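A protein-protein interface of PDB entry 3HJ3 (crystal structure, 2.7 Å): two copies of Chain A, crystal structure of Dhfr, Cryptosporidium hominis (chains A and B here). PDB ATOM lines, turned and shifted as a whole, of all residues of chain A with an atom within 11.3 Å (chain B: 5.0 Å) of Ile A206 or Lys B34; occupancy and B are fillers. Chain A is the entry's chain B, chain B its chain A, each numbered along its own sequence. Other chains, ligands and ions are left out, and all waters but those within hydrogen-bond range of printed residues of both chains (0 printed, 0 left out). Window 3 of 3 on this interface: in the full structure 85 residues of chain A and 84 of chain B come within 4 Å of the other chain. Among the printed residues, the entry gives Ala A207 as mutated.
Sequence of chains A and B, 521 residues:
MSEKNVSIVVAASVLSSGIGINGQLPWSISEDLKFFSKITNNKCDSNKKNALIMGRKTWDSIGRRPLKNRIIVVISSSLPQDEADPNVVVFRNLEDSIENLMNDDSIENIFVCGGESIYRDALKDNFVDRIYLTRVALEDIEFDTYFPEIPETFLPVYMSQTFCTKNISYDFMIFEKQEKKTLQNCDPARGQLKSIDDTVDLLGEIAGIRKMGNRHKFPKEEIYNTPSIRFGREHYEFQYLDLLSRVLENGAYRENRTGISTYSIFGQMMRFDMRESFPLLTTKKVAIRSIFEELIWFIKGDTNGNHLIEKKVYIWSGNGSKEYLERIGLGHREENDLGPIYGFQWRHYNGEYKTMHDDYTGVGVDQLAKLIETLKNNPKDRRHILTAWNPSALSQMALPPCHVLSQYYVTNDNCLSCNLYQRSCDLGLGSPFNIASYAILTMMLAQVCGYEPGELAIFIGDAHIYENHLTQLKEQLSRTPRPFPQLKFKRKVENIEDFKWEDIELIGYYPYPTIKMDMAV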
ATOM      1  N   ASP A 197       0.970 -38.581   7.446  1.00  0.00           N
ATOM      2  CA  ASP A 197       0.294 -37.848   6.404  1.00  0.00           C
ATOM      3  C   ASP A 197      -0.907 -37.174   6.976  1.00  0.00           C
ATOM      4  O   ASP A 197      -1.284 -36.112   6.527  1.00  0.00           O
ATOM      5  CB  ASP A 197      -0.124 -38.779   5.285  1.00  0.00           C
ATOM      6  CG  ASP A 197       0.971 -39.724   4.920  1.00  0.00           C
ATOM      7  OD1 ASP A 197       1.889 -39.268   4.185  1.00  0.00           O
ATOM      8  OD2 ASP A 197       0.928 -40.891   5.413  1.00  0.00           O
ATOM      9  N   ASP A 198      -1.517 -37.794   7.973  1.00  0.00           N
ATOM     10  CA  ASP A 198      -2.634 -37.170   8.626  1.00  0.00           C
ATOM     11  C   ASP A 198      -2.195 -35.890   9.284  1.00  0.00           C
ATOM     12  O   ASP A 198      -2.836 -34.844   9.109  1.00  0.00           O
ATOM     13  CB  ASP A 198      -3.269 -38.112   9.635  1.00  0.00           C
ATOM     14  CG  ASP A 198      -4.120 -39.190   8.968  1.00  0.00           C
ATOM     15  OD1 ASP A 198      -4.645 -40.075   9.712  1.00  0.00           O
ATOM     16  OD2 ASP A 198      -4.258 -39.149   7.706  1.00  0.00           O
ATOM     17  N   THR A 199      -1.098 -35.970  10.033  1.00  0.00           N
ATOM     18  CA  THR A 199      -0.610 -34.846  10.795  1.00  0.00           C
ATOM     19  C   THR A 199      -0.202 -33.751   9.860  1.00  0.00           C
ATOM     20  O   THR A 199      -0.507 -32.597  10.141  1.00  0.00           O
ATOM     21  CB  THR A 199       0.567 -35.211  11.732  1.00  0.00           C
ATOM     22  OG1 THR A 199       0.125 -36.177  12.681  1.00  0.00           O
ATOM     23  CG2 THR A 199       1.049 -34.028  12.512  1.00  0.00           C
ATOM     24  N   VAL A 200       0.495 -34.091   8.774  1.00  0.00           N
ATOM     25  CA  VAL A 200       0.922 -33.079   7.811  1.00  0.00           C
ATOM     26  C   VAL A 200      -0.300 -32.476   7.110  1.00  0.00           C
ATOM     27  O   VAL A 200      -0.304 -31.266   6.787  1.00  0.00           O
ATOM     28  CB  VAL A 200       1.921 -33.623   6.722  1.00  0.00           C
ATOM     29  CG1 VAL A 200       2.409 -32.468   5.785  1.00  0.00           C
ATOM     30  CG2 VAL A 200       3.110 -34.263   7.360  1.00  0.00           C
ATOM     31  N   ASP A 201      -1.321 -33.308   6.867  1.00  0.00           N
ATOM     32  CA  ASP A 201      -2.591 -32.829   6.293  1.00  0.00           C
ATOM     33  C   ASP A 201      -3.312 -31.851   7.252  1.00  0.00           C
ATOM     34  O   ASP A 201      -3.619 -30.700   6.862  1.00  0.00           O
ATOM     35  CB  ASP A 201      -3.501 -33.997   5.873  1.00  0.00           C
ATOM     36  CG  ASP A 201      -2.986 -34.722   4.626  1.00  0.00           C
ATOM     37  OD1 ASP A 201      -3.256 -35.937   4.439  1.00  0.00           O
ATOM     38  OD2 ASP A 201      -2.286 -34.072   3.823  1.00  0.00           O
ATOM     39  N   LEU A 202      -3.557 -32.293   8.500  1.00  0.00           N
ATOM     40  CA  LEU A 202      -4.122 -31.420   9.539  1.00  0.00           C
ATOM     41  C   LEU A 202      -3.345 -30.087   9.659  1.00  0.00           C
ATOM     42  O   LEU A 202      -3.945 -29.009   9.722  1.00  0.00           O
ATOM     43  CB  LEU A 202      -4.176 -32.158  10.869  1.00  0.00           C
ATOM     44  CG  LEU A 202      -5.329 -33.179  11.046  1.00  0.00           C
ATOM     45  CD1 LEU A 202      -6.054 -33.605   9.756  1.00  0.00           C
ATOM     46  CD2 LEU A 202      -4.883 -34.424  11.821  1.00  0.00           C
ATOM     47  N   LEU A 203      -2.016 -30.150   9.612  1.00  0.00           N
ATOM     48  CA  LEU A 203      -1.224 -28.948   9.727  1.00  0.00           C
ATOM     49  C   LEU A 203      -1.492 -28.046   8.576  1.00  0.00           C
ATOM     50  O   LEU A 203      -1.499 -26.837   8.745  1.00  0.00           O
ATOM     51  CB  LEU A 203       0.253 -29.257   9.786  1.00  0.00           C
ATOM     52  CG  LEU A 203       0.893 -29.282  11.179  1.00  0.00           C
ATOM     53  CD1 LEU A 203      -0.080 -29.088  12.409  1.00  0.00           C
ATOM     54  CD2 LEU A 203       1.787 -30.535  11.342  1.00  0.00           C
ATOM     55  N   GLY A 204      -1.718 -28.642   7.405  1.00  0.00           N
ATOM     56  CA  GLY A 204      -1.845 -27.877   6.200  1.00  0.00           C
ATOM     57  C   GLY A 204      -3.132 -27.122   6.305  1.00  0.00           C
ATOM     58  O   GLY A 204      -3.232 -25.939   5.917  1.00  0.00           O
ATOM     59  N   GLU A 205      -4.129 -27.804   6.847  1.00  0.00           N
ATOM     60  CA  GLU A 205      -5.434 -27.180   6.996  1.00  0.00           C
ATOM     61  C   GLU A 205      -5.379 -26.003   7.993  1.00  0.00           C
ATOM     62  O   GLU A 205      -5.931 -24.948   7.735  1.00  0.00           O
ATOM     63  CB  GLU A 205      -6.479 -28.217   7.411  1.00  0.00           C
ATOM     64  CG  GLU A 205      -6.770 -29.263   6.333  1.00  0.00           C
ATOM     65  CD  GLU A 205      -7.491 -30.499   6.892  1.00  0.00           C
ATOM     66  OE1 GLU A 205      -8.069 -30.357   8.000  1.00  0.00           O
ATOM     67  OE2 GLU A 205      -7.477 -31.596   6.240  1.00  0.00           O
ATOM     68  N   ILE A 206      -4.702 -26.191   9.127  1.00  0.00           N
ATOM     69  CA  ILE A 206      -4.609 -25.148  10.129  1.00  0.00           C
ATOM     70  C   ILE A 206      -3.895 -23.941   9.556  1.00  0.00           C
ATOM     71  O   ILE A 206      -4.352 -22.817   9.727  1.00  0.00           O
ATOM     72  CB  ILE A 206      -3.861 -25.645  11.350  1.00  0.00           C
ATOM     73  CG1 ILE A 206      -4.695 -26.651  12.095  1.00  0.00           C
ATOM     74  CG2 ILE A 206      -3.462 -24.514  12.283  1.00  0.00           C
ATOM     75  CD1 ILE A 206      -3.825 -27.475  13.045  1.00  0.00           C
ATOM     76  N   ALA A 207      -2.779 -24.195   8.877  1.00  0.00           N
ATOM     77  CA  ALA A 207      -1.884 -23.149   8.394  1.00  0.00           C
ATOM     78  C   ALA A 207      -2.160 -22.604   6.979  1.00  0.00           C
ATOM     79  O   ALA A 207      -1.828 -21.442   6.699  1.00  0.00           O
ATOM     80  CB  ALA A 207      -0.408 -23.602   8.515  1.00  0.00           C
ATOM     81  N   GLY A 208      -2.731 -23.430   6.095  1.00  0.00           N
ATOM     82  CA  GLY A 208      -2.878 -23.055   4.685  1.00  0.00           C
ATOM     83  C   GLY A 208      -1.528 -22.661   4.057  1.00  0.00           C
ATOM     84  O   GLY A 208      -0.559 -23.432   4.070  1.00  0.00           O
ATOM     85  N   ILE A 209      -1.464 -21.441   3.539  1.00  0.00           N
ATOM     86  CA  ILE A 209      -0.325 -20.884   2.805  1.00  0.00           C
ATOM     87  C   ILE A 209       0.881 -20.675   3.722  1.00  0.00           C
ATOM     88  O   ILE A 209       2.030 -20.565   3.269  1.00  0.00           O
ATOM     89  CB  ILE A 209      -0.731 -19.493   2.153  1.00  0.00           C
ATOM     90  CG1 ILE A 209      -2.091 -19.606   1.455  1.00  0.00           C
ATOM     91  CG2 ILE A 209       0.305 -18.978   1.156  1.00  0.00           C
ATOM     92  CD1 ILE A 209      -2.795 -18.242   1.238  1.00  0.00           C
ATOM     93  N   ARG A 210       0.604 -20.590   5.016  1.00  0.00           N
ATOM     94  CA  ARG A 210       1.628 -20.395   6.019  1.00  0.00           C
ATOM     95  C   ARG A 210       2.572 -21.605   6.214  1.00  0.00           C
ATOM     96  O   ARG A 210       3.638 -21.444   6.812  1.00  0.00           O
ATOM     97  CB  ARG A 210       0.953 -20.029   7.333  1.00  0.00           C
ATOM     98  CG  ARG A 210       0.494 -18.557   7.421  1.00  0.00           C
ATOM     99  CD  ARG A 210      -0.197 -18.272   8.772  1.00  0.00           C
ATOM    100  NE  ARG A 210       0.615 -18.602   9.970  1.00  0.00           N
ATOM    101  CZ  ARG A 210       0.305 -19.558  10.860  1.00  0.00           C
ATOM    102  NH1 ARG A 210      -0.793 -20.302  10.684  1.00  0.00           N
ATOM    103  NH2 ARG A 210       1.091 -19.797  11.923  1.00  0.00           N
ATOM    104  N   LYS A 211       2.200 -22.792   5.726  1.00  0.00           N
ATOM    105  CA  LYS A 211       3.076 -23.958   5.777  1.00  0.00           C
ATOM    106  C   LYS A 211       3.701 -24.166   4.400  1.00  0.00           C
ATOM    107  O   LYS A 211       2.984 -24.473   3.430  1.00  0.00           O
ATOM    108  CB  LYS A 211       2.247 -25.170   6.140  1.00  0.00           C
ATOM    109  CG  LYS A 211       2.897 -26.521   5.974  1.00  0.00           C
ATOM    110  CD  LYS A 211       2.474 -27.396   7.132  1.00  0.00           C
ATOM    111  CE  LYS A 211       2.587 -28.873   6.832  1.00  0.00           C
ATOM    112  NZ  LYS A 211       3.944 -29.224   6.483  1.00  0.00           N
ATOM    113  N   MET A 212       5.025 -24.022   4.297  1.00  0.00           N
ATOM    114  CA  MET A 212       5.724 -24.092   3.016  1.00  0.00           C
ATOM    115  C   MET A 212       5.296 -25.293   2.168  1.00  0.00           C
ATOM    116  O   MET A 212       5.267 -25.209   0.944  1.00  0.00           O
ATOM    117  CB  MET A 212       7.231 -24.091   3.243  1.00  0.00           C
ATOM    118  CG  MET A 212       8.017 -23.976   1.959  1.00  0.00           C
ATOM    119  SD  MET A 212       9.608 -23.132   2.152  1.00  0.00           S
ATOM    120  CE  MET A 212      10.610 -23.825   0.839  1.00  0.00           C
ATOM    121  N   GLY A 213       4.944 -26.399   2.827  1.00  0.00           N
ATOM    122  CA  GLY A 213       4.381 -27.582   2.139  1.00  0.00           C
ATOM    123  C   GLY A 213       3.188 -27.267   1.247  1.00  0.00           C
ATOM    124  O   GLY A 213       3.147 -27.779   0.127  1.00  0.00           O
ATOM    125  N   ASN A 214       2.234 -26.426   1.716  1.00  0.00           N
ATOM    126  CA  ASN A 214       1.083 -25.980   0.860  1.00  0.00           C
ATOM    127  C   ASN A 214       1.510 -25.074  -0.307  1.00  0.00           C
ATOM    128  O   ASN A 214       0.778 -24.883  -1.257  1.00  0.00           O
ATOM    129  CB  ASN A 214      -0.032 -25.334   1.671  1.00  0.00           C
ATOM    130  CG  ASN A 214      -0.822 -26.345   2.479  1.00  0.00           C
ATOM    131  OD1 ASN A 214      -0.377 -26.798   3.508  1.00  0.00           O
ATOM    132  ND2 ASN A 214      -1.995 -26.698   2.011  1.00  0.00           N
ATOM    133  N   LYS A 217       2.651 -27.791  -3.567  1.00  0.00           N
ATOM    134  CA  LYS A 217       1.648 -28.848  -3.592  1.00  0.00           C
ATOM    135  C   LYS A 217       2.107 -29.900  -4.597  1.00  0.00           C
ATOM    136  O   LYS A 217       2.709 -29.566  -5.626  1.00  0.00           O
ATOM    137  CB  LYS A 217       0.297 -28.262  -4.010  1.00  0.00           C
ATOM    138  CG  LYS A 217      -0.835 -28.584  -3.084  1.00  0.00           C
ATOM    139  CD  LYS A 217      -1.690 -27.339  -2.867  1.00  0.00           C
ATOM    140  CE  LYS A 217      -2.221 -27.285  -1.424  1.00  0.00           C
ATOM    141  NZ  LYS A 217      -2.480 -25.878  -0.933  1.00  0.00           N
ATOM    142  N   SER B  30      -3.173 -20.324  19.729  1.00  0.00           N
ATOM    143  CA  SER B  30      -4.421 -20.846  19.188  1.00  0.00           C
ATOM    144  C   SER B  30      -4.165 -21.999  18.223  1.00  0.00           C
ATOM    145  O   SER B  30      -4.840 -23.027  18.275  1.00  0.00           O
ATOM    146  CB  SER B  30      -5.207 -19.737  18.485  1.00  0.00           C
ATOM    147  OG  SER B  30      -4.374 -18.629  18.194  1.00  0.00           O
ATOM    148  N   GLU B  31      -3.185 -21.820  17.343  1.00  0.00           N
ATOM    149  CA  GLU B  31      -2.822 -22.860  16.367  1.00  0.00           C
ATOM    150  C   GLU B  31      -2.639 -24.156  17.103  1.00  0.00           C
ATOM    151  O   GLU B  31      -2.978 -25.208  16.594  1.00  0.00           O
ATOM    152  CB  GLU B  31      -1.540 -22.539  15.579  1.00  0.00           C
ATOM    153  CG  GLU B  31      -1.637 -21.420  14.532  1.00  0.00           C
ATOM    154  CD  GLU B  31      -1.732 -19.989  15.158  1.00  0.00           C
ATOM    155  OE1 GLU B  31      -1.635 -18.980  14.393  1.00  0.00           O
ATOM    156  OE2 GLU B  31      -1.897 -19.861  16.410  1.00  0.00           O
ATOM    157  N   ASP B  32      -2.124 -24.101  18.318  1.00  0.00           N
ATOM    158  CA  ASP B  32      -1.902 -25.348  19.046  1.00  0.00           C
ATOM    159  C   ASP B  32      -3.241 -25.953  19.530  1.00  0.00           C
ATOM    160  O   ASP B  32      -3.417 -27.206  19.470  1.00  0.00           O
ATOM    161  CB  ASP B  32      -0.865 -25.194  20.151  1.00  0.00           C
ATOM    162  CG  ASP B  32      -0.685 -26.477  20.935  1.00  0.00           C
ATOM    163  OD1 ASP B  32      -0.153 -27.443  20.373  1.00  0.00           O
ATOM    164  OD2 ASP B  32      -1.079 -26.558  22.133  1.00  0.00           O
ATOM    165  N   LEU B  33      -4.187 -25.096  19.959  1.00  0.00           N
ATOM    166  CA  LEU B  33      -5.491 -25.591  20.307  1.00  0.00           C
ATOM    167  C   LEU B  33      -6.122 -26.186  19.055  1.00  0.00           C
ATOM    168  O   LEU B  33      -6.717 -27.269  19.106  1.00  0.00           O
ATOM    169  CB  LEU B  33      -6.393 -24.506  20.899  1.00  0.00           C
ATOM    170  CG  LEU B  33      -5.944 -23.963  22.275  1.00  0.00           C
ATOM    171  CD1 LEU B  33      -6.973 -22.991  22.800  1.00  0.00           C
ATOM    172  CD2 LEU B  33      -5.620 -25.059  23.347  1.00  0.00           C
ATOM    173  N   LYS B  34      -5.991 -25.490  17.923  1.00  0.00           N
ATOM    174  CA  LYS B  34      -6.519 -26.004  16.665  1.00  0.00           C
ATOM    175  C   LYS B  34      -5.942 -27.383  16.348  1.00  0.00           C
ATOM    176  O   LYS B  34      -6.709 -28.321  16.012  1.00  0.00           O
ATOM    177  CB  LYS B  34      -6.275 -25.033  15.525  1.00  0.00           C
ATOM    178  CG  LYS B  34      -7.437 -24.094  15.324  1.00  0.00           C
ATOM    179  CD  LYS B  34      -7.281 -23.204  14.068  1.00  0.00           C
ATOM    180  CE  LYS B  34      -7.931 -23.856  12.793  1.00  0.00           C
ATOM    181  NZ  LYS B  34      -9.432 -24.087  12.974  1.00  0.00           N
ATOM    182  N   PHE B  35      -4.614 -27.524  16.491  1.00  0.00           N
ATOM    183  CA  PHE B  35      -3.954 -28.798  16.246  1.00  0.00           C
ATOM    184  C   PHE B  35      -4.523 -29.839  17.170  1.00  0.00           C
ATOM    185  O   PHE B  35      -4.903 -30.961  16.711  1.00  0.00           O
ATOM    186  CB  PHE B  35      -2.446 -28.676  16.411  1.00  0.00           C
ATOM    187  CG  PHE B  35      -1.737 -29.952  16.237  1.00  0.00           C
ATOM    188  CD1 PHE B  35      -1.640 -30.510  14.979  1.00  0.00           C
ATOM    189  CD2 PHE B  35      -1.186 -30.629  17.333  1.00  0.00           C
ATOM    190  CE1 PHE B  35      -0.988 -31.759  14.758  1.00  0.00           C
ATOM    191  CE2 PHE B  35      -0.527 -31.878  17.146  1.00  0.00           C
ATOM    192  CZ  PHE B  35      -0.426 -32.446  15.832  1.00  0.00           C
ATOM    193  N   PHE B  36      -4.632 -29.482  18.457  1.00  0.00           N
ATOM    194  CA  PHE B  36      -5.256 -30.381  19.454  1.00  0.00           C
ATOM    195  C   PHE B  36      -6.677 -30.829  19.031  1.00  0.00           C
ATOM    196  O   PHE B  36      -7.114 -31.962  19.230  1.00  0.00           O
ATOM    197  CB  PHE B  36      -5.287 -29.703  20.852  1.00  0.00           C
ATOM    198  CG  PHE B  36      -5.916 -30.563  21.922  1.00  0.00           C
ATOM    199  CD1 PHE B  36      -7.283 -30.599  22.073  1.00  0.00           C
ATOM    200  CD2 PHE B  36      -5.136 -31.378  22.723  1.00  0.00           C
ATOM    201  CE1 PHE B  36      -7.866 -31.405  22.996  1.00  0.00           C
ATOM    202  CE2 PHE B  36      -5.716 -32.231  23.690  1.00  0.00           C
ATOM    203  CZ  PHE B  36      -7.085 -32.237  23.824  1.00  0.00           C
ATOM    204  N   SER B  37      -7.401 -29.912  18.436  1.00  0.00           N
ATOM    205  CA  SER B  37      -8.736 -30.184  18.030  1.00  0.00           C
ATOM    206  C   SER B  37      -8.722 -31.175  16.871  1.00  0.00           C
ATOM    207  O   SER B  37      -9.440 -32.178  16.928  1.00  0.00           O
ATOM    208  CB  SER B  37      -9.412 -28.865  17.646  1.00  0.00           C
ATOM    209  OG  SER B  37     -10.779 -29.063  17.339  1.00  0.00           O
ATOM    210  N   LYS B  38      -7.909 -30.896  15.830  1.00  0.00           N
ATOM    211  CA  LYS B  38      -7.800 -31.793  14.636  1.00  0.00           C
ATOM    212  C   LYS B  38      -7.347 -33.210  15.008  1.00  0.00           C
ATOM    213  O   LYS B  38      -8.023 -34.159  14.672  1.00  0.00           O
ATOM    214  CB  LYS B  38      -6.900 -31.209  13.550  1.00  0.00           C
ATOM    215  CG  LYS B  38      -7.367 -29.852  12.943  1.00  0.00           C
ATOM    216  CD  LYS B  38      -8.689 -30.047  12.163  1.00  0.00           C
ATOM    217  CE  LYS B  38      -9.289 -28.757  11.639  1.00  0.00           C
ATOM    218  NZ  LYS B  38      -8.411 -28.193  10.596  1.00  0.00           N
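Among the printed residues, merely in contact across the chains: Thr A199 with Phe B35 (3.8 Å), Leu A202 with Lys B38 (3.6 Å), Leu A203 with Phe B35 (3.3 Å), Ile A206 with Lys B34 (3.9 Å) and Ile A206 with Phe B35 (3.5 Å).
Hydrophobic or aromatic side chains of chain B that line the printed part of chain A: Phe B35.
Hydrophobic or aromatic side chains of chain A that line the printed part of chain B: Leu A202, Leu A203 and Ile A206.
Among the printed residues, 7 pairs touch across the chains.
NH2 of Arg A210 lies within salt-bridge range of OE1 of Glu B31, 3.8 Å away.
NZ of Lys B38 lies within salt-bridge range of OE1 of Glu A205 (3.4 Å).
No position is printed for both chains.
Of the 7 pairs that touch across the chains among the printed residues, none has its exchanged pair printed and touching as well.
Ile A206 touches two residues of chain B.
Of chain A, only Ile A206 comes within 4 Å of Lys B34.
No residue of chain A comes within 4 Å of Ser B30.
No residue of chain A comes within 4 Å of Asp B32.
Of chain A, only Thr A199, Leu A203 and Ile A206 come within 4 Å of Phe B35.
No residue of chain A comes within 4 Å of Ser B37.
Of the printed residues of chain B, Leu A203 touches Phe B35.
Of the printed residues of chain B, Glu A205 touches Lys B38.
Printed residues of chain B within 4 Å of Thr A199: Phe B35 (3.8 Å).
Met A212 touches none of the printed residues of chain B.
Asn A214 touches none of the printed residues of chain B.
The nearest residue of chain A that does not touch Lys B34 is Glu A205 (5.5 Å).
The nearest printed residue of chain B that does not touch Leu A202 is Phe B35 (5.0 Å).
OG of Ser B30 sits at hydrogen-bond distance from OE2 of Glu B31 (3.3 Å).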
